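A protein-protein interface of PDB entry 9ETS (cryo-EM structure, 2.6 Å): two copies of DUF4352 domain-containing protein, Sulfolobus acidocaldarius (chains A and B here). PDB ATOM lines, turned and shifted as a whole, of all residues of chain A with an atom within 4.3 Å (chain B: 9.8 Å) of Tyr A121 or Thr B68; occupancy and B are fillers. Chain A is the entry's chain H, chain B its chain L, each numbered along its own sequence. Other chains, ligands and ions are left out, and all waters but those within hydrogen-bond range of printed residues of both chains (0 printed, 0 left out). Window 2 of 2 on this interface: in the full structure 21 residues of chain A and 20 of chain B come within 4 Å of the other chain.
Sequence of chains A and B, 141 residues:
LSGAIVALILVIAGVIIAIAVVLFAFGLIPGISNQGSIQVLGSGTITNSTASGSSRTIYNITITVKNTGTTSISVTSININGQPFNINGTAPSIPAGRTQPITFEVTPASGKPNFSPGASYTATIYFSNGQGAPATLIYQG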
ATOM      1  N   ILE A  80      23.129 -23.838  25.541  1.00  0.00           N
ATOM      2  CA  ILE A  80      22.662 -22.806  24.620  1.00  0.00           C
ATOM      3  C   ILE A  80      22.451 -23.433  23.247  1.00  0.00           C
ATOM      4  O   ILE A  80      23.395 -23.933  22.637  1.00  0.00           O
ATOM      5  CB  ILE A  80      23.621 -21.596  24.557  1.00  0.00           C
ATOM      6  CG1 ILE A  80      23.759 -20.933  25.928  1.00  0.00           C
ATOM      7  CG2 ILE A  80      23.170 -20.603  23.492  1.00  0.00           C
ATOM      8  CD1 ILE A  80      24.777 -19.815  25.983  1.00  0.00           C
ATOM      9  N   ASN A  81      21.199 -23.399  22.765  1.00  0.00           N
ATOM     10  CA  ASN A  81      20.822 -23.850  21.431  1.00  0.00           C
ATOM     11  C   ASN A  81      21.271 -25.299  21.171  1.00  0.00           C
ATOM     12  O   ASN A  81      21.796 -25.633  20.106  1.00  0.00           O
ATOM     13  CB  ASN A  81      21.305 -22.836  20.396  1.00  0.00           C
ATOM     14  CG  ASN A  81      20.227 -22.472  19.408  1.00  0.00           C
ATOM     15  OD1 ASN A  81      19.189 -21.920  19.770  1.00  0.00           O
ATOM     16  ND2 ASN A  81      20.477 -22.786  18.152  1.00  0.00           N
ATOM     17  N   PHE A 115      27.587 -16.490  17.264  1.00  0.00           N
ATOM     18  CA  PHE A 115      26.345 -15.748  17.386  1.00  0.00           C
ATOM     19  C   PHE A 115      26.344 -14.547  16.434  1.00  0.00           C
ATOM     20  O   PHE A 115      27.360 -13.875  16.284  1.00  0.00           O
ATOM     21  CB  PHE A 115      26.143 -15.332  18.841  1.00  0.00           C
ATOM     22  CG  PHE A 115      26.248 -16.444  19.856  1.00  0.00           C
ATOM     23  CD1 PHE A 115      25.259 -17.414  19.958  1.00  0.00           C
ATOM     24  CD2 PHE A 115      27.321 -16.499  20.738  1.00  0.00           C
ATOM     25  CE1 PHE A 115      25.353 -18.425  20.908  1.00  0.00           C
ATOM     26  CE2 PHE A 115      27.418 -17.515  21.684  1.00  0.00           C
ATOM     27  CZ  PHE A 115      26.431 -18.475  21.769  1.00  0.00           C
ATOM     28  N   SER A 116      25.195 -14.282  15.789  1.00  0.00           N
ATOM     29  CA  SER A 116      25.047 -13.180  14.847  1.00  0.00           C
ATOM     30  C   SER A 116      24.212 -12.070  15.480  1.00  0.00           C
ATOM     31  O   SER A 116      23.147 -12.358  16.014  1.00  0.00           O
ATOM     32  CB  SER A 116      24.414 -13.655  13.562  1.00  0.00           C
ATOM     33  OG  SER A 116      23.142 -14.235  13.815  1.00  0.00           O
ATOM     34  N   ALA A 119      20.139 -11.898  16.447  1.00  0.00           N
ATOM     35  CA  ALA A 119      19.501 -13.212  16.381  1.00  0.00           C
ATOM     36  C   ALA A 119      19.139 -13.729  17.779  1.00  0.00           C
ATOM     37  O   ALA A 119      19.759 -13.349  18.776  1.00  0.00           O
ATOM     38  CB  ALA A 119      20.381 -14.181  15.623  1.00  0.00           C
ATOM     39  N   SER A 120      18.145 -14.633  17.830  1.00  0.00           N
ATOM     40  CA  SER A 120      17.637 -15.246  19.053  1.00  0.00           C
ATOM     41  C   SER A 120      18.120 -16.688  19.184  1.00  0.00           C
ATOM     42  O   SER A 120      18.062 -17.453  18.224  1.00  0.00           O
ATOM     43  CB  SER A 120      16.130 -15.233  19.073  1.00  0.00           C
ATOM     44  OG  SER A 120      15.623 -13.913  19.084  1.00  0.00           O
ATOM     45  N   TYR A 121      18.536 -17.070  20.401  1.00  0.00           N
ATOM     46  CA  TYR A 121      19.016 -18.406  20.747  1.00  0.00           C
ATOM     47  C   TYR A 121      18.266 -18.900  21.982  1.00  0.00           C
ATOM     48  O   TYR A 121      17.963 -18.090  22.853  1.00  0.00           O
ATOM     49  CB  TYR A 121      20.532 -18.354  20.988  1.00  0.00           C
ATOM     50  CG  TYR A 121      21.269 -17.850  19.775  1.00  0.00           C
ATOM     51  CD1 TYR A 121      21.568 -18.701  18.719  1.00  0.00           C
ATOM     52  CD2 TYR A 121      21.591 -16.508  19.636  1.00  0.00           C
ATOM     53  CE1 TYR A 121      22.174 -18.233  17.564  1.00  0.00           C
ATOM     54  CE2 TYR A 121      22.201 -16.023  18.487  1.00  0.00           C
ATOM     55  CZ  TYR A 121      22.496 -16.891  17.448  1.00  0.00           C
ATOM     56  OH  TYR A 121      23.077 -16.445  16.297  1.00  0.00           O
ATOM     57  N   THR A 122      17.980 -20.208  22.101  1.00  0.00           N
ATOM     58  CA  THR A 122      17.342 -20.683  23.326  1.00  0.00           C
ATOM     59  C   THR A 122      18.387 -21.201  24.299  1.00  0.00           C
ATOM     60  O   THR A 122      19.034 -22.198  24.024  1.00  0.00           O
ATOM     61  CB  THR A 122      16.297 -21.788  23.113  1.00  0.00           C
ATOM     62  OG1 THR A 122      16.868 -23.024  22.687  1.00  0.00           O
ATOM     63  CG2 THR A 122      15.241 -21.404  22.111  1.00  0.00           C
ATOM     64  N   ALA A 123      18.526 -20.553  25.456  1.00  0.00           N
ATOM     65  CA  ALA A 123      19.197 -21.188  26.575  1.00  0.00           C
ATOM     66  C   ALA A 123      18.221 -22.124  27.288  1.00  0.00           C
ATOM     67  O   ALA A 123      17.024 -21.863  27.323  1.00  0.00           O
ATOM     68  CB  ALA A 123      19.703 -20.128  27.514  1.00  0.00           C
ATOM     69  N   ALA A 135      14.680 -20.412  27.985  1.00  0.00           N
ATOM     70  CA  ALA A 135      14.676 -18.959  27.906  1.00  0.00           C
ATOM     71  C   ALA A 135      15.248 -18.511  26.562  1.00  0.00           C
ATOM     72  O   ALA A 135      16.123 -19.167  26.006  1.00  0.00           O
ATOM     73  CB  ALA A 135      15.491 -18.402  29.043  1.00  0.00           C
ATOM     74  N   THR A 136      14.775 -17.377  26.035  1.00  0.00           N
ATOM     75  CA  THR A 136      15.318 -16.838  24.794  1.00  0.00           C
ATOM     76  C   THR A 136      16.312 -15.734  25.121  1.00  0.00           C
ATOM     77  O   THR A 136      15.985 -14.808  25.861  1.00  0.00           O
ATOM     78  CB  THR A 136      14.217 -16.291  23.874  1.00  0.00           C
ATOM     79  OG1 THR A 136      13.390 -17.378  23.461  1.00  0.00           O
ATOM     80  CG2 THR A 136      14.752 -15.611  22.632  1.00  0.00           C
ATOM     81  N   LEU A 137      17.518 -15.839  24.552  1.00  0.00           N
ATOM     82  CA  LEU A 137      18.542 -14.810  24.642  1.00  0.00           C
ATOM     83  C   LEU A 137      18.700 -14.159  23.272  1.00  0.00           C
ATOM     84  O   LEU A 137      18.778 -14.859  22.271  1.00  0.00           O
ATOM     85  CB  LEU A 137      19.868 -15.446  25.071  1.00  0.00           C
ATOM     86  CG  LEU A 137      19.848 -16.324  26.322  1.00  0.00           C
ATOM     87  CD1 LEU A 137      21.250 -16.832  26.606  1.00  0.00           C
ATOM     88  CD2 LEU A 137      19.324 -15.567  27.533  1.00  0.00           C
ATOM     89  N   TYR A 139      21.323 -11.954  20.989  1.00  0.00           N
ATOM     90  CA  TYR A 139      22.740 -11.623  20.969  1.00  0.00           C
ATOM     91  C   TYR A 139      22.973 -10.148  20.630  1.00  0.00           C
ATOM     92  O   TYR A 139      22.541  -9.667  19.586  1.00  0.00           O
ATOM     93  CB  TYR A 139      23.494 -12.585  20.051  1.00  0.00           C
ATOM     94  CG  TYR A 139      24.966 -12.275  19.950  1.00  0.00           C
ATOM     95  CD1 TYR A 139      25.847 -12.610  20.971  1.00  0.00           C
ATOM     96  CD2 TYR A 139      25.476 -11.630  18.833  1.00  0.00           C
ATOM     97  CE1 TYR A 139      27.203 -12.323  20.879  1.00  0.00           C
ATOM     98  CE2 TYR A 139      26.823 -11.320  18.733  1.00  0.00           C
ATOM     99  CZ  TYR A 139      27.689 -11.668  19.759  1.00  0.00           C
ATOM    100  OH  TYR A 139      29.014 -11.341  19.661  1.00  0.00           O
ATOM    101  N   SER B  33      14.238 -28.105  21.557  1.00  0.00           N
ATOM    102  CA  SER B  33      14.124 -26.664  21.386  1.00  0.00           C
ATOM    103  C   SER B  33      15.459 -26.093  20.907  1.00  0.00           C
ATOM    104  O   SER B  33      16.491 -26.236  21.563  1.00  0.00           O
ATOM    105  CB  SER B  33      13.569 -25.975  22.623  1.00  0.00           C
ATOM    106  OG  SER B  33      14.500 -25.934  23.693  1.00  0.00           O
ATOM    107  N   ASN B  34      15.431 -25.475  19.725  1.00  0.00           N
ATOM    108  CA  ASN B  34      16.630 -25.178  18.970  1.00  0.00           C
ATOM    109  C   ASN B  34      16.242 -24.080  17.987  1.00  0.00           C
ATOM    110  O   ASN B  34      15.701 -24.381  16.926  1.00  0.00           O
ATOM    111  CB  ASN B  34      17.122 -26.471  18.308  1.00  0.00           C
ATOM    112  CG  ASN B  34      18.459 -26.363  17.612  1.00  0.00           C
ATOM    113  OD1 ASN B  34      18.831 -25.313  17.098  1.00  0.00           O
ATOM    114  ND2 ASN B  34      19.191 -27.463  17.570  1.00  0.00           N
ATOM    115  N   GLN B  35      16.496 -22.822  18.359  1.00  0.00           N
ATOM    116  CA  GLN B  35      16.115 -21.698  17.519  1.00  0.00           C
ATOM    117  C   GLN B  35      17.123 -21.514  16.386  1.00  0.00           C
ATOM    118  O   GLN B  35      18.254 -21.996  16.438  1.00  0.00           O
ATOM    119  CB  GLN B  35      15.996 -20.416  18.346  1.00  0.00           C
ATOM    120  CG  GLN B  35      14.736 -20.359  19.196  1.00  0.00           C
ATOM    121  CD  GLN B  35      14.429 -18.961  19.687  1.00  0.00           C
ATOM    122  OE1 GLN B  35      14.401 -18.681  20.887  1.00  0.00           O
ATOM    123  NE2 GLN B  35      14.186 -18.060  18.747  1.00  0.00           N
ATOM    124  N   GLY B  36      16.710 -20.765  15.363  1.00  0.00           N
ATOM    125  CA  GLY B  36      17.618 -20.506  14.263  1.00  0.00           C
ATOM    126  C   GLY B  36      17.628 -21.648  13.253  1.00  0.00           C
ATOM    127  O   GLY B  36      17.407 -22.816  13.568  1.00  0.00           O
ATOM    128  N   SER B  37      17.931 -21.257  12.016  1.00  0.00           N
ATOM    129  CA  SER B  37      17.636 -22.032  10.828  1.00  0.00           C
ATOM    130  C   SER B  37      18.490 -21.503   9.682  1.00  0.00           C
ATOM    131  O   SER B  37      19.106 -20.442   9.799  1.00  0.00           O
ATOM    132  CB  SER B  37      16.171 -21.890  10.502  1.00  0.00           C
ATOM    133  OG  SER B  37      15.831 -20.525  10.292  1.00  0.00           O
ATOM    134  N   ILE B  38      18.490 -22.228   8.565  1.00  0.00           N
ATOM    135  CA  ILE B  38      18.975 -21.630   7.339  1.00  0.00           C
ATOM    136  C   ILE B  38      17.872 -20.792   6.697  1.00  0.00           C
ATOM    137  O   ILE B  38      16.753 -21.257   6.503  1.00  0.00           O
ATOM    138  CB  ILE B  38      19.608 -22.677   6.410  1.00  0.00           C
ATOM    139  CG1 ILE B  38      20.902 -23.169   7.066  1.00  0.00           C
ATOM    140  CG2 ILE B  38      19.843 -22.042   5.056  1.00  0.00           C
ATOM    141  CD1 ILE B  38      21.952 -23.705   6.122  1.00  0.00           C
ATOM    142  N   GLN B  39      18.238 -19.548   6.359  1.00  0.00           N
ATOM    143  CA  GLN B  39      17.404 -18.577   5.667  1.00  0.00           C
ATOM    144  C   GLN B  39      17.957 -18.322   4.265  1.00  0.00           C
ATOM    145  O   GLN B  39      19.170 -18.213   4.084  1.00  0.00           O
ATOM    146  CB  GLN B  39      17.388 -17.276   6.470  1.00  0.00           C
ATOM    147  CG  GLN B  39      16.654 -17.403   7.797  1.00  0.00           C
ATOM    148  CD  GLN B  39      16.696 -16.146   8.634  1.00  0.00           C
ATOM    149  OE1 GLN B  39      17.182 -15.099   8.207  1.00  0.00           O
ATOM    150  NE2 GLN B  39      16.187 -16.239   9.853  1.00  0.00           N
ATOM    151  N   VAL B  40      17.060 -18.208   3.275  1.00  0.00           N
ATOM    152  CA  VAL B  40      17.447 -17.990   1.888  1.00  0.00           C
ATOM    153  C   VAL B  40      17.094 -16.555   1.500  1.00  0.00           C
ATOM    154  O   VAL B  40      15.941 -16.153   1.634  1.00  0.00           O
ATOM    155  CB  VAL B  40      16.782 -19.035   0.968  1.00  0.00           C
ATOM    156  CG1 VAL B  40      17.049 -18.764  -0.498  1.00  0.00           C
ATOM    157  CG2 VAL B  40      17.214 -20.446   1.317  1.00  0.00           C
ATOM    158  N   LEU B  41      18.087 -15.792   1.011  1.00  0.00           N
ATOM    159  CA  LEU B  41      17.958 -14.350   0.826  1.00  0.00           C
ATOM    160  C   LEU B  41      17.932 -13.962  -0.656  1.00  0.00           C
ATOM    161  O   LEU B  41      18.861 -14.267  -1.402  1.00  0.00           O
ATOM    162  CB  LEU B  41      19.113 -13.654   1.550  1.00  0.00           C
ATOM    163  CG  LEU B  41      19.279 -13.984   3.034  1.00  0.00           C
ATOM    164  CD1 LEU B  41      20.475 -13.247   3.619  1.00  0.00           C
ATOM    165  CD2 LEU B  41      18.015 -13.673   3.822  1.00  0.00           C
ATOM    166  N   VAL B  65      22.607 -17.486   1.217  1.00  0.00           N
ATOM    167  CA  VAL B  65      22.135 -18.307   2.322  1.00  0.00           C
ATOM    168  C   VAL B  65      22.720 -17.787   3.635  1.00  0.00           C
ATOM    169  O   VAL B  65      23.905 -17.477   3.705  1.00  0.00           O
ATOM    170  CB  VAL B  65      22.520 -19.778   2.078  1.00  0.00           C
ATOM    171  CG1 VAL B  65      22.050 -20.665   3.208  1.00  0.00           C
ATOM    172  CG2 VAL B  65      21.949 -20.293   0.769  1.00  0.00           C
ATOM    173  N   LYS B  66      21.893 -17.723   4.686  1.00  0.00           N
ATOM    174  CA  LYS B  66      22.305 -17.250   6.000  1.00  0.00           C
ATOM    175  C   LYS B  66      21.975 -18.308   7.056  1.00  0.00           C
ATOM    176  O   LYS B  66      20.808 -18.600   7.303  1.00  0.00           O
ATOM    177  CB  LYS B  66      21.577 -15.933   6.273  1.00  0.00           C
ATOM    178  CG  LYS B  66      21.774 -15.328   7.653  1.00  0.00           C
ATOM    179  CD  LYS B  66      21.028 -14.026   7.789  1.00  0.00           C
ATOM    180  CE  LYS B  66      21.193 -13.364   9.142  1.00  0.00           C
ATOM    181  NZ  LYS B  66      20.368 -12.137   9.261  1.00  0.00           N
ATOM    182  N   ASN B  67      23.002 -18.885   7.686  1.00  0.00           N
ATOM    183  CA  ASN B  67      22.796 -19.842   8.757  1.00  0.00           C
ATOM    184  C   ASN B  67      22.729 -19.083  10.083  1.00  0.00           C
ATOM    185  O   ASN B  67      23.748 -18.589  10.556  1.00  0.00           O
ATOM    186  CB  ASN B  67      23.916 -20.881   8.724  1.00  0.00           C
ATOM    187  CG  ASN B  67      23.799 -21.941   9.793  1.00  0.00           C
ATOM    188  OD1 ASN B  67      22.871 -21.936  10.593  1.00  0.00           O
ATOM    189  ND2 ASN B  67      24.721 -22.880   9.808  1.00  0.00           N
ATOM    190  N   THR B  68      21.539 -19.014  10.696  1.00  0.00           N
ATOM    191  CA  THR B  68      21.357 -18.315  11.967  1.00  0.00           C
ATOM    192  C   THR B  68      21.545 -19.223  13.188  1.00  0.00           C
ATOM    193  O   THR B  68      21.540 -18.740  14.317  1.00  0.00           O
ATOM    194  CB  THR B  68      20.000 -17.607  12.043  1.00  0.00           C
ATOM    195  OG1 THR B  68      18.950 -18.553  11.866  1.00  0.00           O
ATOM    196  CG2 THR B  68      19.833 -16.525  11.003  1.00  0.00           C
ATOM    197  N   GLY B  69      21.710 -20.533  12.978  1.00  0.00           N
ATOM    198  CA  GLY B  69      21.940 -21.471  14.070  1.00  0.00           C
ATOM    199  C   GLY B  69      23.385 -21.478  14.578  1.00  0.00           C
ATOM    200  O   GLY B  69      24.245 -20.741  14.092  1.00  0.00           O
ATOM    201  N   THR B  70      23.649 -22.372  15.544  1.00  0.00           N
ATOM    202  CA  THR B  70      24.939 -22.488  16.222  1.00  0.00           C
ATOM    203  C   THR B  70      25.782 -23.656  15.692  1.00  0.00           C
ATOM    204  O   THR B  70      26.846 -23.947  16.242  1.00  0.00           O
ATOM    205  CB  THR B  70      24.764 -22.606  17.744  1.00  0.00           C
ATOM    206  OG1 THR B  70      23.891 -23.705  18.013  1.00  0.00           O
ATOM    207  CG2 THR B  70      24.232 -21.342  18.384  1.00  0.00           C
ATOM    208  N   THR B  71      25.321 -24.325  14.621  1.00  0.00           N
ATOM    209  CA  THR B  71      25.986 -25.506  14.059  1.00  0.00           C
ATOM    210  C   THR B  71      26.066 -25.432  12.535  1.00  0.00           C
ATOM    211  O   THR B  71      25.197 -24.861  11.888  1.00  0.00           O
ATOM    212  CB  THR B  71      25.262 -26.809  14.432  1.00  0.00           C
ATOM    213  OG1 THR B  71      23.896 -26.748  14.015  1.00  0.00           O
ATOM    214  CG2 THR B  71      25.353 -27.132  15.907  1.00  0.00           C
ATOM    215  N   SER B  72      27.100 -26.063  11.962  1.00  0.00           N
ATOM    216  CA  SER B  72      27.246 -26.183  10.518  1.00  0.00           C
ATOM    217  C   SER B  72      26.175 -27.108   9.932  1.00  0.00           C
ATOM    218  O   SER B  72      25.868 -28.141  10.517  1.00  0.00           O
ATOM    219  CB  SER B  72      28.622 -26.669  10.175  1.00  0.00           C
ATOM    220  OG  SER B  72      28.832 -26.572   8.781  1.00  0.00           O
ATOM    221  N   ILE B  73      25.649 -26.749   8.750  1.00  0.00           N
ATOM    222  CA  ILE B  73      24.517 -27.411   8.097  1.00  0.00           C
ATOM    223  C   ILE B  73      24.847 -27.590   6.610  1.00  0.00           C
ATOM    224  O   ILE B  73      25.704 -26.884   6.097  1.00  0.00           O
ATOM    225  CB  ILE B  73      23.223 -26.597   8.351  1.00  0.00           C
ATOM    226  CG1 ILE B  73      22.734 -26.774   9.790  1.00  0.00           C
ATOM    227  CG2 ILE B  73      22.097 -26.920   7.382  1.00  0.00           C
ATOM    228  CD1 ILE B  73      21.907 -25.620  10.315  1.00  0.00           C
ATOM    229  N   ILE B  94      27.205 -24.725   5.115  1.00  0.00           N
ATOM    230  CA  ILE B  94      27.176 -23.347   5.576  1.00  0.00           C
ATOM    231  C   ILE B  94      27.569 -23.337   7.056  1.00  0.00           C
ATOM    232  O   ILE B  94      26.846 -23.894   7.880  1.00  0.00           O
ATOM    233  CB  ILE B  94      25.779 -22.719   5.344  1.00  0.00           C
ATOM    234  CG1 ILE B  94      25.224 -22.911   3.926  1.00  0.00           C
ATOM    235  CG2 ILE B  94      25.831 -21.239   5.681  1.00  0.00           C
ATOM    236  CD1 ILE B  94      24.558 -24.240   3.638  1.00  0.00           C
ATOM    237  N   PRO B  95      28.703 -22.706   7.452  1.00  0.00           N
ATOM    238  CA  PRO B  95      29.099 -22.620   8.861  1.00  0.00           C
ATOM    239  C   PRO B  95      28.086 -21.842   9.695  1.00  0.00           C
ATOM    240  O   PRO B  95      27.294 -21.060   9.173  1.00  0.00           O
ATOM    241  CB  PRO B  95      30.434 -21.856   8.829  1.00  0.00           C
ATOM    242  CG  PRO B  95      30.947 -22.041   7.415  1.00  0.00           C
ATOM    243  CD  PRO B  95      29.689 -22.063   6.574  1.00  0.00           C
ATOM    244  N   ALA B  96      28.123 -22.057  11.014  1.00  0.00           N
ATOM    245  CA  ALA B  96      27.267 -21.349  11.959  1.00  0.00           C
ATOM    246  C   ALA B  96      27.419 -19.825  11.836  1.00  0.00           C
ATOM    247  O   ALA B  96      28.515 -19.320  11.590  1.00  0.00           O
ATOM    248  CB  ALA B  96      27.610 -21.810  13.348  1.00  0.00           C
ATOM    249  N   GLY B  97      26.304 -19.097  12.000  1.00  0.00           N
ATOM    250  CA  GLY B  97      26.274 -17.640  12.074  1.00  0.00           C
ATOM    251  C   GLY B  97      26.699 -16.882  10.811  1.00  0.00           C
ATOM    252  O   GLY B  97      26.859 -15.663  10.875  1.00  0.00           O
ATOM    253  N   ARG B  98      26.859 -17.567   9.667  1.00  0.00           N
ATOM    254  CA  ARG B  98      27.480 -16.979   8.483  1.00  0.00           C
ATOM    255  C   ARG B  98      26.485 -16.765   7.337  1.00  0.00           C
ATOM    256  O   ARG B  98      25.593 -17.583   7.108  1.00  0.00           O
ATOM    257  CB  ARG B  98      28.649 -17.867   8.043  1.00  0.00           C
ATOM    258  CG  ARG B  98      29.619 -17.172   7.103  1.00  0.00           C
ATOM    259  CD  ARG B  98      30.949 -17.886   6.951  1.00  0.00           C
ATOM    260  NE  ARG B  98      31.644 -18.042   8.229  1.00  0.00           N
ATOM    261  CZ  ARG B  98      32.325 -17.092   8.869  1.00  0.00           C
ATOM    262  NH1 ARG B  98      32.906 -17.370  10.024  1.00  0.00           N
ATOM    263  NH2 ARG B  98      32.434 -15.875   8.361  1.00  0.00           N
ATOM    264  N   THR B  99      26.665 -15.653   6.603  1.00  0.00           N
ATOM    265  CA  THR B  99      25.963 -15.375   5.352  1.00  0.00           C
ATOM    266  C   THR B  99      26.921 -15.603   4.182  1.00  0.00           C
ATOM    267  O   THR B  99      28.039 -15.095   4.199  1.00  0.00           O
ATOM    268  CB  THR B  99      25.434 -13.934   5.288  1.00  0.00           C
ATOM    269  OG1 THR B  99      24.642 -13.662   6.444  1.00  0.00           O
ATOM    270  CG2 THR B  99      24.595 -13.657   4.058  1.00  0.00           C
ATOM    271  N   GLN B 100      26.486 -16.361   3.161  1.00  0.00           N
ATOM    272  CA  GLN B 100      27.325 -16.697   2.016  1.00  0.00           C
ATOM    273  C   GLN B 100      26.496 -16.799   0.740  1.00  0.00           C
ATOM    274  O   GLN B 100      25.368 -17.284   0.765  1.00  0.00           O
ATOM    275  CB  GLN B 100      27.945 -18.090   2.162  1.00  0.00           C
ATOM    276  CG  GLN B 100      28.904 -18.280   3.329  1.00  0.00           C
ATOM    277  CD  GLN B 100      29.525 -19.654   3.242  1.00  0.00           C
ATOM    278  OE1 GLN B 100      29.056 -20.612   3.859  1.00  0.00           O
ATOM    279  NE2 GLN B 100      30.579 -19.769   2.451  1.00  0.00           N
ATOM    280  N   ASN B 129      18.894 -30.552   8.450  1.00  0.00           N
ATOM    281  CA  ASN B 129      17.914 -30.448   9.528  1.00  0.00           C
ATOM    282  C   ASN B 129      16.592 -31.174   9.237  1.00  0.00           C
ATOM    283  O   ASN B 129      15.806 -31.413  10.155  1.00  0.00           O
ATOM    284  CB  ASN B 129      17.513 -28.987   9.752  1.00  0.00           C
ATOM    285  CG  ASN B 129      18.646 -28.096  10.217  1.00  0.00           C
ATOM    286  OD1 ASN B 129      19.603 -28.572  10.824  1.00  0.00           O
ATOM    287  ND2 ASN B 129      18.537 -26.803   9.950  1.00  0.00           N
ATOM    288  N   GLN B 131      14.453 -29.403   7.810  1.00  0.00           N
ATOM    289  CA  GLN B 131      13.910 -28.089   7.474  1.00  0.00           C
ATOM    290  C   GLN B 131      14.142 -27.779   5.989  1.00  0.00           C
ATOM    291  O   GLN B 131      15.232 -28.014   5.464  1.00  0.00           O
ATOM    292  CB  GLN B 131      14.598 -27.043   8.358  1.00  0.00           C
ATOM    293  CG  GLN B 131      14.104 -25.608   8.171  1.00  0.00           C
ATOM    294  CD  GLN B 131      15.197 -24.583   7.955  1.00  0.00           C
ATOM    295  OE1 GLN B 131      16.310 -24.712   8.465  1.00  0.00           O
ATOM    296  NE2 GLN B 131      14.897 -23.534   7.198  1.00  0.00           N
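No position is printed for both chains.
Of the 9 pairs that touch across the chains among the printed residues, none has its exchanged pair printed and touching as well.
The backbone carbonyl oxygen (O) of Ser B33 sits at hydrogen-bond distance from the side-chain hydroxyl (OG1) of Thr A122, at 3.4 Å.
The side-chain amide nitrogen of Asn A81 is in hydrogen-bond range of the side-chain amide oxygen of Asn B34, at 3.2 Å.
The backbone carbonyl oxygen of Gln B35 is in hydrogen-bond range of the side-chain amide nitrogen of Asn A81, at 2.9 Å.
The side-chain amide oxygen of Gln B35 lies within hydrogen-bond range of the side-chain hydroxyl of Thr A136 (3.1 Å).
The backbone carbonyl oxygen (O) of Thr B68 lies close to the side-chain hydroxyl (OH) of Tyr A121.
Of the 27 printed residues of chain B, 5 touch a printed residue of chain A.
Printed residues of chain B that touch a printed residue of chain A: Ser B33, Asn B34, Gln B35, Thr B68 and Thr B70.
Of the 13 printed residues of chain A, 5 touch a printed residue of chain B.
Of chain B, only Thr B68 (3.3 Å) and Thr B70 (3.8 Å) come within 4 Å of Tyr A121.
Thr B68 touches just one residue of chain A: Tyr A121 (3.3 Å).
Ser A120 touches just one residue of chain B: Gln B35.
No residue of chain B comes within 4 Å of Leu A137.
Printed residues of chain B within 4 Å of Asn A81: Asn B34 (3.2 Å), Gln B35 (2.9 Å) and Thr B70 (3.5 Å).
Of the printed residues of chain A, Thr B70 touches Asn A81 (3.5 Å) and Tyr A121 (3.8 Å).
Printed residues of chain A within 4 Å of Asn B34: Asn A81 (3.2 Å).
Of the printed residues of chain A, Gln B35 touches Asn A81, Ser A120, Thr A122 and Thr A136.
Printed residues of chain A within 4 Å of Ser B33: Thr A122.
Gln B131 touches none of the printed residues of chain A.
The nearest printed residue of chain A that does not touch Gln B35 is Tyr A121 (4.02 Å).
O of Ser B37 lies within hydrogen-bond range of OG1 of Thr B68 (2.8 Å).
The backbone NH of Asn A81 is in hydrogen-bond range of the backbone carbonyl oxygen of Thr A122.
The backbone NH (N) of Ser A116 sits at hydrogen-bond distance from the side-chain hydroxyl (OH) of Tyr A121 (3.1 Å).
The backbone carbonyl oxygen (O) of Tyr A121 is in hydrogen-bond range of the backbone NH (N) of Leu A137 (2.9 Å).
Among the printed residues, pairs that only touch across the chains: Asn A81 with Thr B70 (3.5 Å), Ser A120 with Gln B35 (3.4 Å), Tyr A121 with Thr B70 (3.8 Å) and Thr A122 with Gln B35 (3.1 Å).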
